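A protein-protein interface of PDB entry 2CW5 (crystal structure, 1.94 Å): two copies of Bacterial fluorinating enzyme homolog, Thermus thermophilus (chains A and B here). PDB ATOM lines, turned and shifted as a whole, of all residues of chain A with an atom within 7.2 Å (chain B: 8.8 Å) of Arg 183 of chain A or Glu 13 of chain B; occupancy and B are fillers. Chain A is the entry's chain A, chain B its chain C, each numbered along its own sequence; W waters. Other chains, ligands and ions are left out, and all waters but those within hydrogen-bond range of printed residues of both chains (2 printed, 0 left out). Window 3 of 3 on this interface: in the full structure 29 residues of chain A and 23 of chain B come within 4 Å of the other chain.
The backbone carbonyl oxygen (O) of Leu 12 of chain B sits close to the backbone NH (N) of Ala 39 of chain A (3.3 Å). NH2 of Arg 47 of chain A is in hydrogen-bond range of O of Glu 13 of chain B. The side-chain carboxylate (OD1) of Asp 14 of chain B lies within salt-bridge range of the guanidinium group (NH2) of Arg 47 of chain A, 2.4 Å away. The guanidinium group (NE) of Arg 183 of chain A sits at hydrogen-bond distance from the backbone carbonyl oxygen (O) of Phe 10 of chain B. The guanidinium group of Arg 183 of chain A is in salt-bridge range of the side-chain carboxylate of Asp 14 of chain B, at 2.6 Å. O of Leu 36 of chain A sits close to O of Asp 14 of chain B, 3.2 Å away.
Arg 183 of chain A touches four residues of chain B. Glu 13 of chain B touches five residues of chain A. Asp 182 of chain A touches none of the printed residues of chain B. Of the printed residues of chain A, Asp 14 of chain B touches Leu 36, Ala 37, Arg 47 and Arg 183. Printed residues of chain B within 4 Å of Arg 47 of chain A: Glu 13 (3.4 Å) and Asp 14 (2.4 Å). Printed residues of chain B within 4 Å of Leu 40 of chain A: Glu 13. Ala 39 of chain B touches none of the printed residues of chain A. Gly 11 of chain B touches none of the printed residues of chain A. The nearest residue of chain B that does not touch Arg 183 of chain A is Asp 9 of chain B (4.4 Å).
The backbone NH (N) of Ser 8 of chain A is in hydrogen-bond range of the backbone carbonyl oxygen (O) of Ala 37 of chain A (3.0 Å). The side-chain hydroxyl of Ser 8 of chain A lies within hydrogen-bond range of a ring nitrogen (ND1) of His 38 of chain A, at 2.7 Å. NE of Arg 47 of chain A lies close to O of Phe 181 of chain A (3.0 Å). The backbone NH of Phe 10 of chain B is in hydrogen-bond range of the side-chain hydroxyl of Ser 8 of chain B.
Water W1 lies within hydrogen-bond range of the backbone carbonyl oxygen of Leu 36 of chain A, the backbone carbonyl oxygen of Asp 14 of chain B and the backbone NH of Val 17 of chain B. Water W2 bridges N of His 38 of chain A (2.8 Å) and O of Leu 12 of chain B (2.9 Å).
Positions printed for both chains: 8, 38, 39, 40 and 41.
Printed residues of chain B that touch a printed residue of chain A: Phe 10, Leu 12, Glu 13, Asp 14, Pro 15 and Tyr 16. Hydrophobic or aromatic side chains of chain B that line the printed part of chain A: Leu 12, Pro 15 and Tyr 16. Among the printed residues, 18 pairs touch across the chains.
Leu 36 of chain A touches Pro 15 of chain B (O to CA, 3.2 Å). CB of Ala 37 of chain A touches O of Leu 12 of chain B (3.6 Å). CB of Ala 37 of chain A touches O of Glu 13 of chain B, 3.8 Å away. Ala 37 of chain A touches Asp 14 of chain B. N of His 38 of chain A touches O of Leu 12 of chain B (3.8 Å). Pro 15 of chain B touches Ala 51 of chain A (CG to O, 3.6 Å). Glu 54 of chain A touches Pro 15 of chain B. Glu 54 of chain A touches Tyr 16 of chain B (OE2 to CE1, 3.4 Å). Arg 183 of chain A touches Glu 13 of chain B. Tyr 16 of chain B touches Arg 183 of chain A.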
ATOM      1  N   LEU A   7      -8.912 -10.792 -14.916  1.00  0.00           N
ATOM      2  CA  LEU A   7      -9.962 -11.558 -15.583  1.00  0.00           C
ATOM      3  C   LEU A   7      -9.456 -12.922 -16.066  1.00  0.00           C
ATOM      4  O   LEU A   7      -8.299 -13.062 -16.471  1.00  0.00           O
ATOM      5  CB  LEU A   7     -10.507 -10.759 -16.773  1.00  0.00           C
ATOM      6  CG  LEU A   7     -11.614 -11.415 -17.607  1.00  0.00           C
ATOM      7  CD1 LEU A   7     -12.620 -10.376 -18.025  1.00  0.00           C
ATOM      8  CD2 LEU A   7     -11.019 -12.088 -18.820  1.00  0.00           C
ATOM      9  N   SER A   8     -10.321 -13.931 -16.009  1.00  0.00           N
ATOM     10  CA  SER A   8      -9.962 -15.266 -16.478  1.00  0.00           C
ATOM     11  C   SER A   8     -11.202 -16.148 -16.580  1.00  0.00           C
ATOM     12  O   SER A   8     -12.313 -15.738 -16.219  1.00  0.00           O
ATOM     13  CB  SER A   8      -8.961 -15.934 -15.526  1.00  0.00           C
ATOM     14  OG  SER A   8      -9.633 -16.565 -14.445  1.00  0.00           O
ATOM     15  N   LEU A  36     -12.137  -8.854 -12.242  1.00  0.00           N
ATOM     16  CA  LEU A  36     -13.132  -8.428 -13.225  1.00  0.00           C
ATOM     17  C   LEU A  36     -14.177  -9.547 -13.243  1.00  0.00           C
ATOM     18  O   LEU A  36     -15.373  -9.303 -13.073  1.00  0.00           O
ATOM     19  CB  LEU A  36     -12.471  -8.256 -14.601  1.00  0.00           C
ATOM     20  CG  LEU A  36     -11.609  -6.987 -14.697  1.00  0.00           C
ATOM     21  CD1 LEU A  36     -10.616  -7.061 -15.858  1.00  0.00           C
ATOM     22  CD2 LEU A  36     -12.541  -5.790 -14.860  1.00  0.00           C
ATOM     23  N   ALA A  37     -13.703 -10.778 -13.416  1.00  0.00           N
ATOM     24  CA  ALA A  37     -14.544 -11.974 -13.427  1.00  0.00           C
ATOM     25  C   ALA A  37     -13.639 -13.173 -13.675  1.00  0.00           C
ATOM     26  O   ALA A  37     -12.628 -13.058 -14.370  1.00  0.00           O
ATOM     27  CB  ALA A  37     -15.594 -11.893 -14.530  1.00  0.00           C
ATOM     28  N   HIS A  38     -13.998 -14.314 -13.100  1.00  0.00           N
ATOM     29  CA  HIS A  38     -13.224 -15.539 -13.285  1.00  0.00           C
ATOM     30  C   HIS A  38     -14.101 -16.701 -13.730  1.00  0.00           C
ATOM     31  O   HIS A  38     -13.601 -17.789 -14.057  1.00  0.00           O
ATOM     32  CB  HIS A  38     -12.493 -15.891 -11.991  1.00  0.00           C
ATOM     33  CG  HIS A  38     -11.389 -14.937 -11.665  1.00  0.00           C
ATOM     34  ND1 HIS A  38     -10.272 -14.805 -12.461  1.00  0.00           N
ATOM     35  CD2 HIS A  38     -11.266 -14.010 -10.684  1.00  0.00           C
ATOM     36  CE1 HIS A  38      -9.507 -13.837 -11.986  1.00  0.00           C
ATOM     37  NE2 HIS A  38     -10.088 -13.337 -10.908  1.00  0.00           N
ATOM     38  N   ALA A  39     -15.407 -16.466 -13.762  1.00  0.00           N
ATOM     39  CA  ALA A  39     -16.339 -17.512 -14.173  1.00  0.00           C
ATOM     40  C   ALA A  39     -16.817 -17.349 -15.613  1.00  0.00           C
ATOM     41  O   ALA A  39     -17.910 -17.798 -15.970  1.00  0.00           O
ATOM     42  CB  ALA A  39     -17.535 -17.561 -13.219  1.00  0.00           C
ATOM     43  N   LEU A  40     -16.009 -16.699 -16.443  1.00  0.00           N
ATOM     44  CA  LEU A  40     -16.377 -16.547 -17.847  1.00  0.00           C
ATOM     45  C   LEU A  40     -16.431 -17.957 -18.419  1.00  0.00           C
ATOM     46  O   LEU A  40     -15.706 -18.843 -17.956  1.00  0.00           O
ATOM     47  CB  LEU A  40     -15.321 -15.733 -18.608  1.00  0.00           C
ATOM     48  CG  LEU A  40     -15.327 -14.216 -18.404  1.00  0.00           C
ATOM     49  CD1 LEU A  40     -14.114 -13.599 -19.079  1.00  0.00           C
ATOM     50  CD2 LEU A  40     -16.609 -13.634 -18.980  1.00  0.00           C
ATOM     51  N   PRO A  41     -17.289 -18.191 -19.425  1.00  0.00           N
ATOM     52  CA  PRO A  41     -17.382 -19.528 -20.016  1.00  0.00           C
ATOM     53  C   PRO A  41     -16.002 -20.002 -20.458  1.00  0.00           C
ATOM     54  O   PRO A  41     -15.263 -19.270 -21.112  1.00  0.00           O
ATOM     55  CB  PRO A  41     -18.329 -19.320 -21.198  1.00  0.00           C
ATOM     56  CG  PRO A  41     -19.220 -18.220 -20.723  1.00  0.00           C
ATOM     57  CD  PRO A  41     -18.235 -17.264 -20.071  1.00  0.00           C
ATOM     58  N   ARG A  47     -16.629 -13.707 -25.501  1.00  0.00           N
ATOM     59  CA  ARG A  47     -17.272 -13.275 -24.264  1.00  0.00           C
ATOM     60  C   ARG A  47     -16.283 -12.497 -23.393  1.00  0.00           C
ATOM     61  O   ARG A  47     -16.618 -11.471 -22.812  1.00  0.00           O
ATOM     62  CB  ARG A  47     -17.779 -14.497 -23.495  1.00  0.00           C
ATOM     63  CG  ARG A  47     -18.456 -14.162 -22.175  1.00  0.00           C
ATOM     64  CD  ARG A  47     -19.781 -13.464 -22.392  1.00  0.00           C
ATOM     65  NE  ARG A  47     -20.295 -12.943 -21.134  1.00  0.00           N
ATOM     66  CZ  ARG A  47     -19.821 -11.857 -20.533  1.00  0.00           C
ATOM     67  NH1 ARG A  47     -18.830 -11.162 -21.085  1.00  0.00           N
ATOM     68  NH2 ARG A  47     -20.317 -11.481 -19.365  1.00  0.00           N
ATOM     69  N   ALA A  51     -16.232  -8.513 -22.189  1.00  0.00           N
ATOM     70  CA  ALA A  51     -16.180  -8.122 -20.781  1.00  0.00           C
ATOM     71  C   ALA A  51     -15.146  -7.015 -20.609  1.00  0.00           C
ATOM     72  O   ALA A  51     -15.371  -6.039 -19.891  1.00  0.00           O
ATOM     73  CB  ALA A  51     -15.817  -9.319 -19.914  1.00  0.00           C
ATOM     74  N   GLU A  54     -16.514  -3.797 -22.011  1.00  0.00           N
ATOM     75  CA  GLU A  54     -17.506  -3.231 -21.088  1.00  0.00           C
ATOM     76  C   GLU A  54     -16.894  -2.431 -19.947  1.00  0.00           C
ATOM     77  O   GLU A  54     -17.380  -1.361 -19.585  1.00  0.00           O
ATOM     78  CB  GLU A  54     -18.333  -4.341 -20.434  1.00  0.00           C
ATOM     79  CG  GLU A  54     -19.352  -5.032 -21.298  1.00  0.00           C
ATOM     80  CD  GLU A  54     -20.146  -6.048 -20.494  1.00  0.00           C
ATOM     81  OE1 GLU A  54     -19.624  -7.160 -20.236  1.00  0.00           O
ATOM     82  OE2 GLU A  54     -21.281  -5.720 -20.103  1.00  0.00           O
ATOM     83  N   PHE A 181     -23.002 -13.440 -25.596  1.00  0.00           N
ATOM     84  CA  PHE A 181     -24.224 -13.385 -24.789  1.00  0.00           C
ATOM     85  C   PHE A 181     -23.880 -13.087 -23.340  1.00  0.00           C
ATOM     86  O   PHE A 181     -22.736 -13.262 -22.931  1.00  0.00           O
ATOM     87  CB  PHE A 181     -24.944 -14.735 -24.825  1.00  0.00           C
ATOM     88  CG  PHE A 181     -25.346 -15.167 -26.192  1.00  0.00           C
ATOM     89  CD1 PHE A 181     -26.493 -14.651 -26.788  1.00  0.00           C
ATOM     90  CD2 PHE A 181     -24.569 -16.077 -26.897  1.00  0.00           C
ATOM     91  CE1 PHE A 181     -26.861 -15.037 -28.073  1.00  0.00           C
ATOM     92  CE2 PHE A 181     -24.930 -16.470 -28.186  1.00  0.00           C
ATOM     93  CZ  PHE A 181     -26.083 -15.945 -28.773  1.00  0.00           C
ATOM     94  N   ASP A 182     -24.864 -12.628 -22.565  1.00  0.00           N
ATOM     95  CA  ASP A 182     -24.624 -12.387 -21.147  1.00  0.00           C
ATOM     96  C   ASP A 182     -25.281 -13.550 -20.408  1.00  0.00           C
ATOM     97  O   ASP A 182     -25.811 -14.460 -21.045  1.00  0.00           O
ATOM     98  CB  ASP A 182     -25.195 -11.039 -20.681  1.00  0.00           C
ATOM     99  CG  ASP A 182     -26.700 -10.956 -20.800  1.00  0.00           C
ATOM    100  OD1 ASP A 182     -27.357 -11.999 -21.001  1.00  0.00           O
ATOM    101  OD2 ASP A 182     -27.224  -9.831 -20.679  1.00  0.00           O
ATOM    102  N   ARG A 183     -25.256 -13.523 -19.079  1.00  0.00           N
ATOM    103  CA  ARG A 183     -25.816 -14.615 -18.284  1.00  0.00           C
ATOM    104  C   ARG A 183     -27.304 -14.896 -18.457  1.00  0.00           C
ATOM    105  O   ARG A 183     -27.753 -16.014 -18.211  1.00  0.00           O
ATOM    106  CB  ARG A 183     -25.508 -14.395 -16.796  1.00  0.00           C
ATOM    107  CG  ARG A 183     -26.079 -13.122 -16.193  1.00  0.00           C
ATOM    108  CD  ARG A 183     -25.609 -12.964 -14.745  1.00  0.00           C
ATOM    109  NE  ARG A 183     -26.164 -11.781 -14.091  1.00  0.00           N
ATOM    110  CZ  ARG A 183     -26.029 -10.537 -14.544  1.00  0.00           C
ATOM    111  NH1 ARG A 183     -26.568  -9.526 -13.878  1.00  0.00           N
ATOM    112  NH2 ARG A 183     -25.362 -10.303 -15.666  1.00  0.00           N
ATOM    113  N   PHE A 184     -28.069 -13.900 -18.888  1.00  0.00           N
ATOM    114  CA  PHE A 184     -29.505 -14.086 -19.069  1.00  0.00           C
ATOM    115  C   PHE A 184     -29.900 -14.516 -20.479  1.00  0.00           C
ATOM    116  O   PHE A 184     -31.068 -14.799 -20.745  1.00  0.00           O
ATOM    117  CB  PHE A 184     -30.243 -12.801 -18.693  1.00  0.00           C
ATOM    118  CG  PHE A 184     -29.976 -12.347 -17.285  1.00  0.00           C
ATOM    119  CD1 PHE A 184     -30.283 -13.172 -16.205  1.00  0.00           C
ATOM    120  CD2 PHE A 184     -29.400 -11.105 -17.037  1.00  0.00           C
ATOM    121  CE1 PHE A 184     -30.022 -12.764 -14.893  1.00  0.00           C
ATOM    122  CE2 PHE A 184     -29.134 -10.690 -15.728  1.00  0.00           C
ATOM    123  CZ  PHE A 184     -29.446 -11.522 -14.658  1.00  0.00           C
ATOM    124  N   GLY A 185     -28.928 -14.580 -21.379  1.00  0.00           N
ATOM    125  CA  GLY A 185     -29.238 -14.983 -22.735  1.00  0.00           C
ATOM    126  C   GLY A 185     -29.428 -13.808 -23.677  1.00  0.00           C
ATOM    127  O   GLY A 185     -29.811 -14.000 -24.829  1.00  0.00           O
ATOM    128  N   ASN A 186     -29.183 -12.591 -23.195  1.00  0.00           N
ATOM    129  CA  ASN A 186     -29.303 -11.421 -24.055  1.00  0.00           C
ATOM    130  C   ASN A 186     -28.173 -11.532 -25.069  1.00  0.00           C
ATOM    131  O   ASN A 186     -27.046 -11.880 -24.715  1.00  0.00           O
ATOM    132  CB  ASN A 186     -29.141 -10.117 -23.260  1.00  0.00           C
ATOM    133  CG  ASN A 186     -30.251  -9.900 -22.248  1.00  0.00           C
ATOM    134  OD1 ASN A 186     -31.425 -10.141 -22.533  1.00  0.00           O
ATOM    135  ND2 ASN A 186     -29.885  -9.425 -21.061  1.00  0.00           N
ATOM    136  N   SER A 239     -34.935 -15.551 -22.446  1.00  0.00           N
ATOM    137  CA  SER A 239     -33.591 -15.714 -22.990  1.00  0.00           C
ATOM    138  C   SER A 239     -33.593 -15.738 -24.509  1.00  0.00           C
ATOM    139  O   SER A 239     -34.012 -16.720 -25.125  1.00  0.00           O
ATOM    140  CB  SER A 239     -32.960 -17.007 -22.480  1.00  0.00           C
ATOM    141  OG  SER A 239     -31.736 -17.265 -23.150  1.00  0.00           O
ATOM    142  N   ARG A 241     -31.108 -15.986 -26.479  1.00  0.00           N
ATOM    143  CA  ARG A 241     -30.200 -17.042 -26.922  1.00  0.00           C
ATOM    144  C   ARG A 241     -30.938 -18.368 -27.096  1.00  0.00           C
ATOM    145  O   ARG A 241     -30.872 -19.001 -28.151  1.00  0.00           O
ATOM    146  CB  ARG A 241     -29.072 -17.212 -25.903  1.00  0.00           C
ATOM    147  CG  ARG A 241     -28.010 -18.221 -26.302  1.00  0.00           C
ATOM    148  CD  ARG A 241     -26.927 -18.301 -25.235  1.00  0.00           C
ATOM    149  NE  ARG A 241     -25.799 -19.128 -25.648  1.00  0.00           N
ATOM    150  CZ  ARG A 241     -24.713 -19.329 -24.908  1.00  0.00           C
ATOM    151  NH1 ARG A 241     -24.607 -18.762 -23.713  1.00  0.00           N
ATOM    152  NH2 ARG A 241     -23.731 -20.096 -25.362  1.00  0.00           N
ATOM    153  N   SER B   8     -24.531  -7.449  -4.060  1.00  0.00           N
ATOM    154  CA  SER B   8     -25.282  -7.402  -5.308  1.00  0.00           C
ATOM    155  C   SER B   8     -25.650  -8.801  -5.753  1.00  0.00           C
ATOM    156  O   SER B   8     -25.274  -9.783  -5.117  1.00  0.00           O
ATOM    157  CB  SER B   8     -24.447  -6.755  -6.415  1.00  0.00           C
ATOM    158  OG  SER B   8     -23.524  -7.690  -6.952  1.00  0.00           O
ATOM    159  N   ASP B   9     -26.403  -8.881  -6.848  1.00  0.00           N
ATOM    160  CA  ASP B   9     -26.766 -10.165  -7.431  1.00  0.00           C
ATOM    161  C   ASP B   9     -26.153 -10.187  -8.836  1.00  0.00           C
ATOM    162  O   ASP B   9     -26.632 -10.899  -9.715  1.00  0.00           O
ATOM    163  CB  ASP B   9     -28.289 -10.317  -7.517  1.00  0.00           C
ATOM    164  CG  ASP B   9     -28.933  -9.303  -8.457  1.00  0.00           C
ATOM    165  OD1 ASP B   9     -28.250  -8.344  -8.867  1.00  0.00           O
ATOM    166  OD2 ASP B   9     -30.132  -9.467  -8.780  1.00  0.00           O
ATOM    167  N   PHE B  10     -25.094  -9.402  -9.032  1.00  0.00           N
ATOM    168  CA  PHE B  10     -24.429  -9.306 -10.336  1.00  0.00           C
ATOM    169  C   PHE B  10     -23.782 -10.603 -10.816  1.00  0.00           C
ATOM    170  O   PHE B  10     -23.567 -10.775 -12.010  1.00  0.00           O
ATOM    171  CB  PHE B  10     -23.366  -8.195 -10.339  1.00  0.00           C
ATOM    172  CG  PHE B  10     -23.923  -6.804 -10.175  1.00  0.00           C
ATOM    173  CD1 PHE B  10     -25.279  -6.546 -10.351  1.00  0.00           C
ATOM    174  CD2 PHE B  10     -23.076  -5.743  -9.868  1.00  0.00           C
ATOM    175  CE1 PHE B  10     -25.786  -5.248 -10.224  1.00  0.00           C
ATOM    176  CE2 PHE B  10     -23.571  -4.443  -9.740  1.00  0.00           C
ATOM    177  CZ  PHE B  10     -24.928  -4.196  -9.919  1.00  0.00           C
ATOM    178  N   GLY B  11     -23.459 -11.505  -9.898  1.00  0.00           N
ATOM    179  CA  GLY B  11     -22.857 -12.760 -10.313  1.00  0.00           C
ATOM    180  C   GLY B  11     -21.355 -12.709 -10.526  1.00  0.00           C
ATOM    181  O   GLY B  11     -20.726 -11.663 -10.358  1.00  0.00           O
ATOM    182  N   LEU B  12     -20.793 -13.846 -10.937  1.00  0.00           N
ATOM    183  CA  LEU B  12     -19.357 -13.995 -11.143  1.00  0.00           C
ATOM    184  C   LEU B  12     -18.930 -14.103 -12.605  1.00  0.00           C
ATOM    185  O   LEU B  12     -17.747 -14.284 -12.891  1.00  0.00           O
ATOM    186  CB  LEU B  12     -18.879 -15.251 -10.408  1.00  0.00           C
ATOM    187  CG  LEU B  12     -19.474 -15.484  -9.020  1.00  0.00           C
ATOM    188  CD1 LEU B  12     -19.076 -16.862  -8.519  1.00  0.00           C
ATOM    189  CD2 LEU B  12     -19.008 -14.405  -8.066  1.00  0.00           C
ATOM    190  N   GLU B  13     -19.882 -14.002 -13.526  1.00  0.00           N
ATOM    191  CA  GLU B  13     -19.573 -14.126 -14.949  1.00  0.00           C
ATOM    192  C   GLU B  13     -19.300 -12.810 -15.664  1.00  0.00           C
ATOM    193  O   GLU B  13     -18.638 -12.788 -16.702  1.00  0.00           O
ATOM    194  CB  GLU B  13     -20.713 -14.847 -15.671  1.00  0.00           C
ATOM    195  CG  GLU B  13     -20.839 -16.316 -15.341  1.00  0.00           C
ATOM    196  CD  GLU B  13     -21.980 -16.975 -16.091  1.00  0.00           C
ATOM    197  OE1 GLU B  13     -23.150 -16.712 -15.748  1.00  0.00           O
ATOM    198  OE2 GLU B  13     -21.706 -17.750 -17.029  1.00  0.00           O
ATOM    199  N   ASP B  14     -19.807 -11.718 -15.106  1.00  0.00           N
ATOM    200  CA  ASP B  14     -19.648 -10.401 -15.708  1.00  0.00           C
ATOM    201  C   ASP B  14     -18.732  -9.513 -14.878  1.00  0.00           C
ATOM    202  O   ASP B  14     -18.456  -9.800 -13.714  1.00  0.00           O
ATOM    203  CB  ASP B  14     -21.016  -9.730 -15.830  1.00  0.00           C
ATOM    204  CG  ASP B  14     -22.026 -10.592 -16.558  1.00  0.00           C
ATOM    205  OD1 ASP B  14     -21.956 -10.676 -17.802  1.00  0.00           O
ATOM    206  OD2 ASP B  14     -22.889 -11.193 -15.886  1.00  0.00           O
ATOM    207  N   PRO B  15     -18.245  -8.417 -15.473  1.00  0.00           N
ATOM    208  CA  PRO B  15     -17.357  -7.493 -14.764  1.00  0.00           C
ATOM    209  C   PRO B  15     -18.125  -6.362 -14.068  1.00  0.00           C
ATOM    210  O   PRO B  15     -17.541  -5.343 -13.719  1.00  0.00           O
ATOM    211  CB  PRO B  15     -16.464  -6.971 -15.881  1.00  0.00           C
ATOM    212  CG  PRO B  15     -17.448  -6.833 -17.009  1.00  0.00           C
ATOM    213  CD  PRO B  15     -18.268  -8.117 -16.918  1.00  0.00           C
ATOM    214  N   TYR B  16     -19.423  -6.545 -13.854  1.00  0.00           N
ATOM    215  CA  TYR B  16     -20.229  -5.495 -13.222  1.00  0.00           C
ATOM    216  C   TYR B  16     -19.747  -5.087 -11.832  1.00  0.00           C
ATOM    217  O   TYR B  16     -19.660  -3.897 -11.524  1.00  0.00           O
ATOM    218  CB  TYR B  16     -21.699  -5.914 -13.161  1.00  0.00           C
ATOM    219  CG  TYR B  16     -22.264  -6.332 -14.499  1.00  0.00           C
ATOM    220  CD1 TYR B  16     -21.914  -5.656 -15.669  1.00  0.00           C
ATOM    221  CD2 TYR B  16     -23.155  -7.400 -14.596  1.00  0.00           C
ATOM    222  CE1 TYR B  16     -22.435  -6.035 -16.907  1.00  0.00           C
ATOM    223  CE2 TYR B  16     -23.685  -7.787 -15.828  1.00  0.00           C
ATOM    224  CZ  TYR B  16     -23.319  -7.103 -16.977  1.00  0.00           C
ATOM    225  OH  TYR B  16     -23.823  -7.500 -18.193  1.00  0.00           O
ATOM    226  N   VAL B  17     -19.422  -6.060 -10.988  1.00  0.00           N
ATOM    227  CA  VAL B  17     -18.947  -5.724  -9.646  1.00  0.00           C
ATOM    228  C   VAL B  17     -17.682  -4.873  -9.733  1.00  0.00           C
ATOM    229  O   VAL B  17     -17.550  -3.864  -9.038  1.00  0.00           O
ATOM    230  CB  VAL B  17     -18.647  -7.000  -8.806  1.00  0.00           C
ATOM    231  CG1 VAL B  17     -17.949  -6.619  -7.499  1.00  0.00           C
ATOM    232  CG2 VAL B  17     -19.954  -7.740  -8.493  1.00  0.00           C
ATOM    233  N   HIS B  38     -21.947 -11.360  -3.811  1.00  0.00           N
ATOM    234  CA  HIS B  38     -22.257 -11.004  -5.192  1.00  0.00           C
ATOM    235  C   HIS B  38     -22.822 -12.170  -6.000  1.00  0.00           C
ATOM    236  O   HIS B  38     -23.379 -11.973  -7.082  1.00  0.00           O
ATOM    237  CB  HIS B  38     -21.005 -10.452  -5.897  1.00  0.00           C
ATOM    238  CG  HIS B  38     -20.547  -9.130  -5.362  1.00  0.00           C
ATOM    239  ND1 HIS B  38     -21.342  -8.004  -5.390  1.00  0.00           N
ATOM    240  CD2 HIS B  38     -19.407  -8.771  -4.726  1.00  0.00           C
ATOM    241  CE1 HIS B  38     -20.713  -7.009  -4.790  1.00  0.00           C
ATOM    242  NE2 HIS B  38     -19.536  -7.449  -4.376  1.00  0.00           N
ATOM    243  N   ALA B  39     -22.676 -13.383  -5.480  1.00  0.00           N
ATOM    244  CA  ALA B  39     -23.177 -14.567  -6.170  1.00  0.00           C
ATOM    245  C   ALA B  39     -24.563 -14.961  -5.660  1.00  0.00           C
ATOM    246  O   ALA B  39     -24.871 -16.142  -5.548  1.00  0.00           O
ATOM    247  CB  ALA B  39     -22.197 -15.733  -5.992  1.00  0.00           C
ATOM    248  N   LEU B  40     -25.388 -13.967  -5.348  1.00  0.00           N
ATOM    249  CA  LEU B  40     -26.741 -14.219  -4.850  1.00  0.00           C
ATOM    250  C   LEU B  40     -27.698 -14.467  -6.009  1.00  0.00           C
ATOM    251  O   LEU B  40     -27.503 -13.941  -7.107  1.00  0.00           O
ATOM    252  CB  LEU B  40     -27.240 -13.020  -4.036  1.00  0.00           C
ATOM    253  CG  LEU B  40     -26.423 -12.631  -2.799  1.00  0.00           C
ATOM    254  CD1 LEU B  40     -26.996 -11.358  -2.197  1.00  0.00           C
ATOM    255  CD2 LEU B  40     -26.440 -13.764  -1.781  1.00  0.00           C
ATOM    256  N   PRO B  41     -28.757 -15.264  -5.780  1.00  0.00           N
ATOM    257  CA  PRO B  41     -29.709 -15.533  -6.862  1.00  0.00           C
ATOM    258  C   PRO B  41     -30.253 -14.223  -7.427  1.00  0.00           C
ATOM    259  O   PRO B  41     -30.662 -13.332  -6.680  1.00  0.00           O
ATOM    260  CB  PRO B  41     -30.788 -16.370  -6.175  1.00  0.00           C
ATOM    261  CG  PRO B  41     -30.026 -17.084  -5.095  1.00  0.00           C
ATOM    262  CD  PRO B  41     -29.136 -15.989  -4.553  1.00  0.00           C
ATOM    263  N   PRO B  42     -30.248 -14.079  -8.759  1.00  0.00           N
ATOM    264  CA  PRO B  42     -30.752 -12.851  -9.378  1.00  0.00           C
ATOM    265  C   PRO B  42     -32.162 -12.481  -8.926  1.00  0.00           C
ATOM    266  O   PRO B  42     -33.038 -13.341  -8.827  1.00  0.00           O
ATOM    267  CB  PRO B  42     -30.674 -13.167 -10.869  1.00  0.00           C
ATOM    268  CG  PRO B  42     -29.463 -14.049 -10.943  1.00  0.00           C
ATOM    269  CD  PRO B  42     -29.686 -14.985  -9.776  1.00  0.00           C
ATOM    270  N   GLN B  43     -32.362 -11.196  -8.640  1.00  0.00           N
ATOM    271  CA  GLN B  43     -33.651 -10.665  -8.198  1.00  0.00           C
ATOM    272  C   GLN B  43     -34.200 -11.223  -6.882  1.00  0.00           C
ATOM    273  O   GLN B  43     -35.300 -10.853  -6.479  1.00  0.00           O
ATOM    274  CB  GLN B  43     -34.713 -10.871  -9.283  1.00  0.00           C
ATOM    275  CG  GLN B  43     -34.427 -10.177 -10.604  1.00  0.00           C
ATOM    276  CD  GLN B  43     -35.618 -10.230 -11.548  1.00  0.00           C
ATOM    277  OE1 GLN B  43     -36.709  -9.761 -11.215  1.00  0.00           O
ATOM    278  NE2 GLN B  43     -35.415 -10.807 -12.730  1.00  0.00           N
ATOM    279  N   VAL B  68     -27.111  -3.616  -4.483  1.00  0.00           N
ATOM    280  CA  VAL B  68     -27.840  -3.530  -5.744  1.00  0.00           C
ATOM    281  C   VAL B  68     -28.433  -4.867  -6.169  1.00  0.00           C
ATOM    282  O   VAL B  68     -27.712  -5.761  -6.621  1.00  0.00           O
ATOM    283  CB  VAL B  68     -26.928  -3.011  -6.873  1.00  0.00           C
ATOM    284  CG1 VAL B  68     -27.735  -2.859  -8.166  1.00  0.00           C
ATOM    285  CG2 VAL B  68     -26.307  -1.679  -6.472  1.00  0.00           C
ATOM    286  N   THR B 131     -29.353   1.559 -18.180  1.00  0.00           N
ATOM    287  CA  THR B 131     -29.084   0.151 -18.451  1.00  0.00           C
ATOM    288  C   THR B 131     -28.142  -0.476 -17.419  1.00  0.00           C
ATOM    289  O   THR B 131     -27.899  -1.684 -17.448  1.00  0.00           O
ATOM    290  CB  THR B 131     -28.463  -0.037 -19.858  1.00  0.00           C
ATOM    291  OG1 THR B 131     -27.288   0.776 -19.978  1.00  0.00           O
ATOM    292  CG2 THR B 131     -29.459   0.363 -20.941  1.00  0.00           C
ATOM    293  N   PHE B 132     -27.624   0.344 -16.508  1.00  0.00           N
ATOM    294  CA  PHE B 132     -26.696  -0.132 -15.484  1.00  0.00           C
ATOM    295  C   PHE B 132     -26.705   0.856 -14.314  1.00  0.00           C
ATOM    296  O   PHE B 132     -25.747   1.601 -14.112  1.00  0.00           O
ATOM    297  CB  PHE B 132     -25.283  -0.226 -16.088  1.00  0.00           C
ATOM    298  CG  PHE B 132     -24.291  -0.996 -15.243  1.00  0.00           C
ATOM    299  CD1 PHE B 132     -24.589  -1.368 -13.933  1.00  0.00           C
ATOM    300  CD2 PHE B 132     -23.045  -1.333 -15.766  1.00  0.00           C
ATOM    301  CE1 PHE B 132     -23.660  -2.065 -13.154  1.00  0.00           C
ATOM    302  CE2 PHE B 132     -22.109  -2.025 -15.002  1.00  0.00           C
ATOM    303  CZ  PHE B 132     -22.419  -2.393 -13.688  1.00  0.00           C
HETATM  304  O   HOH W   1     -16.925  -8.193 -11.479  1.00  0.00           O
HETATM  305  O   HOH W   2     -15.655 -14.539 -10.842  1.00  0.00           O
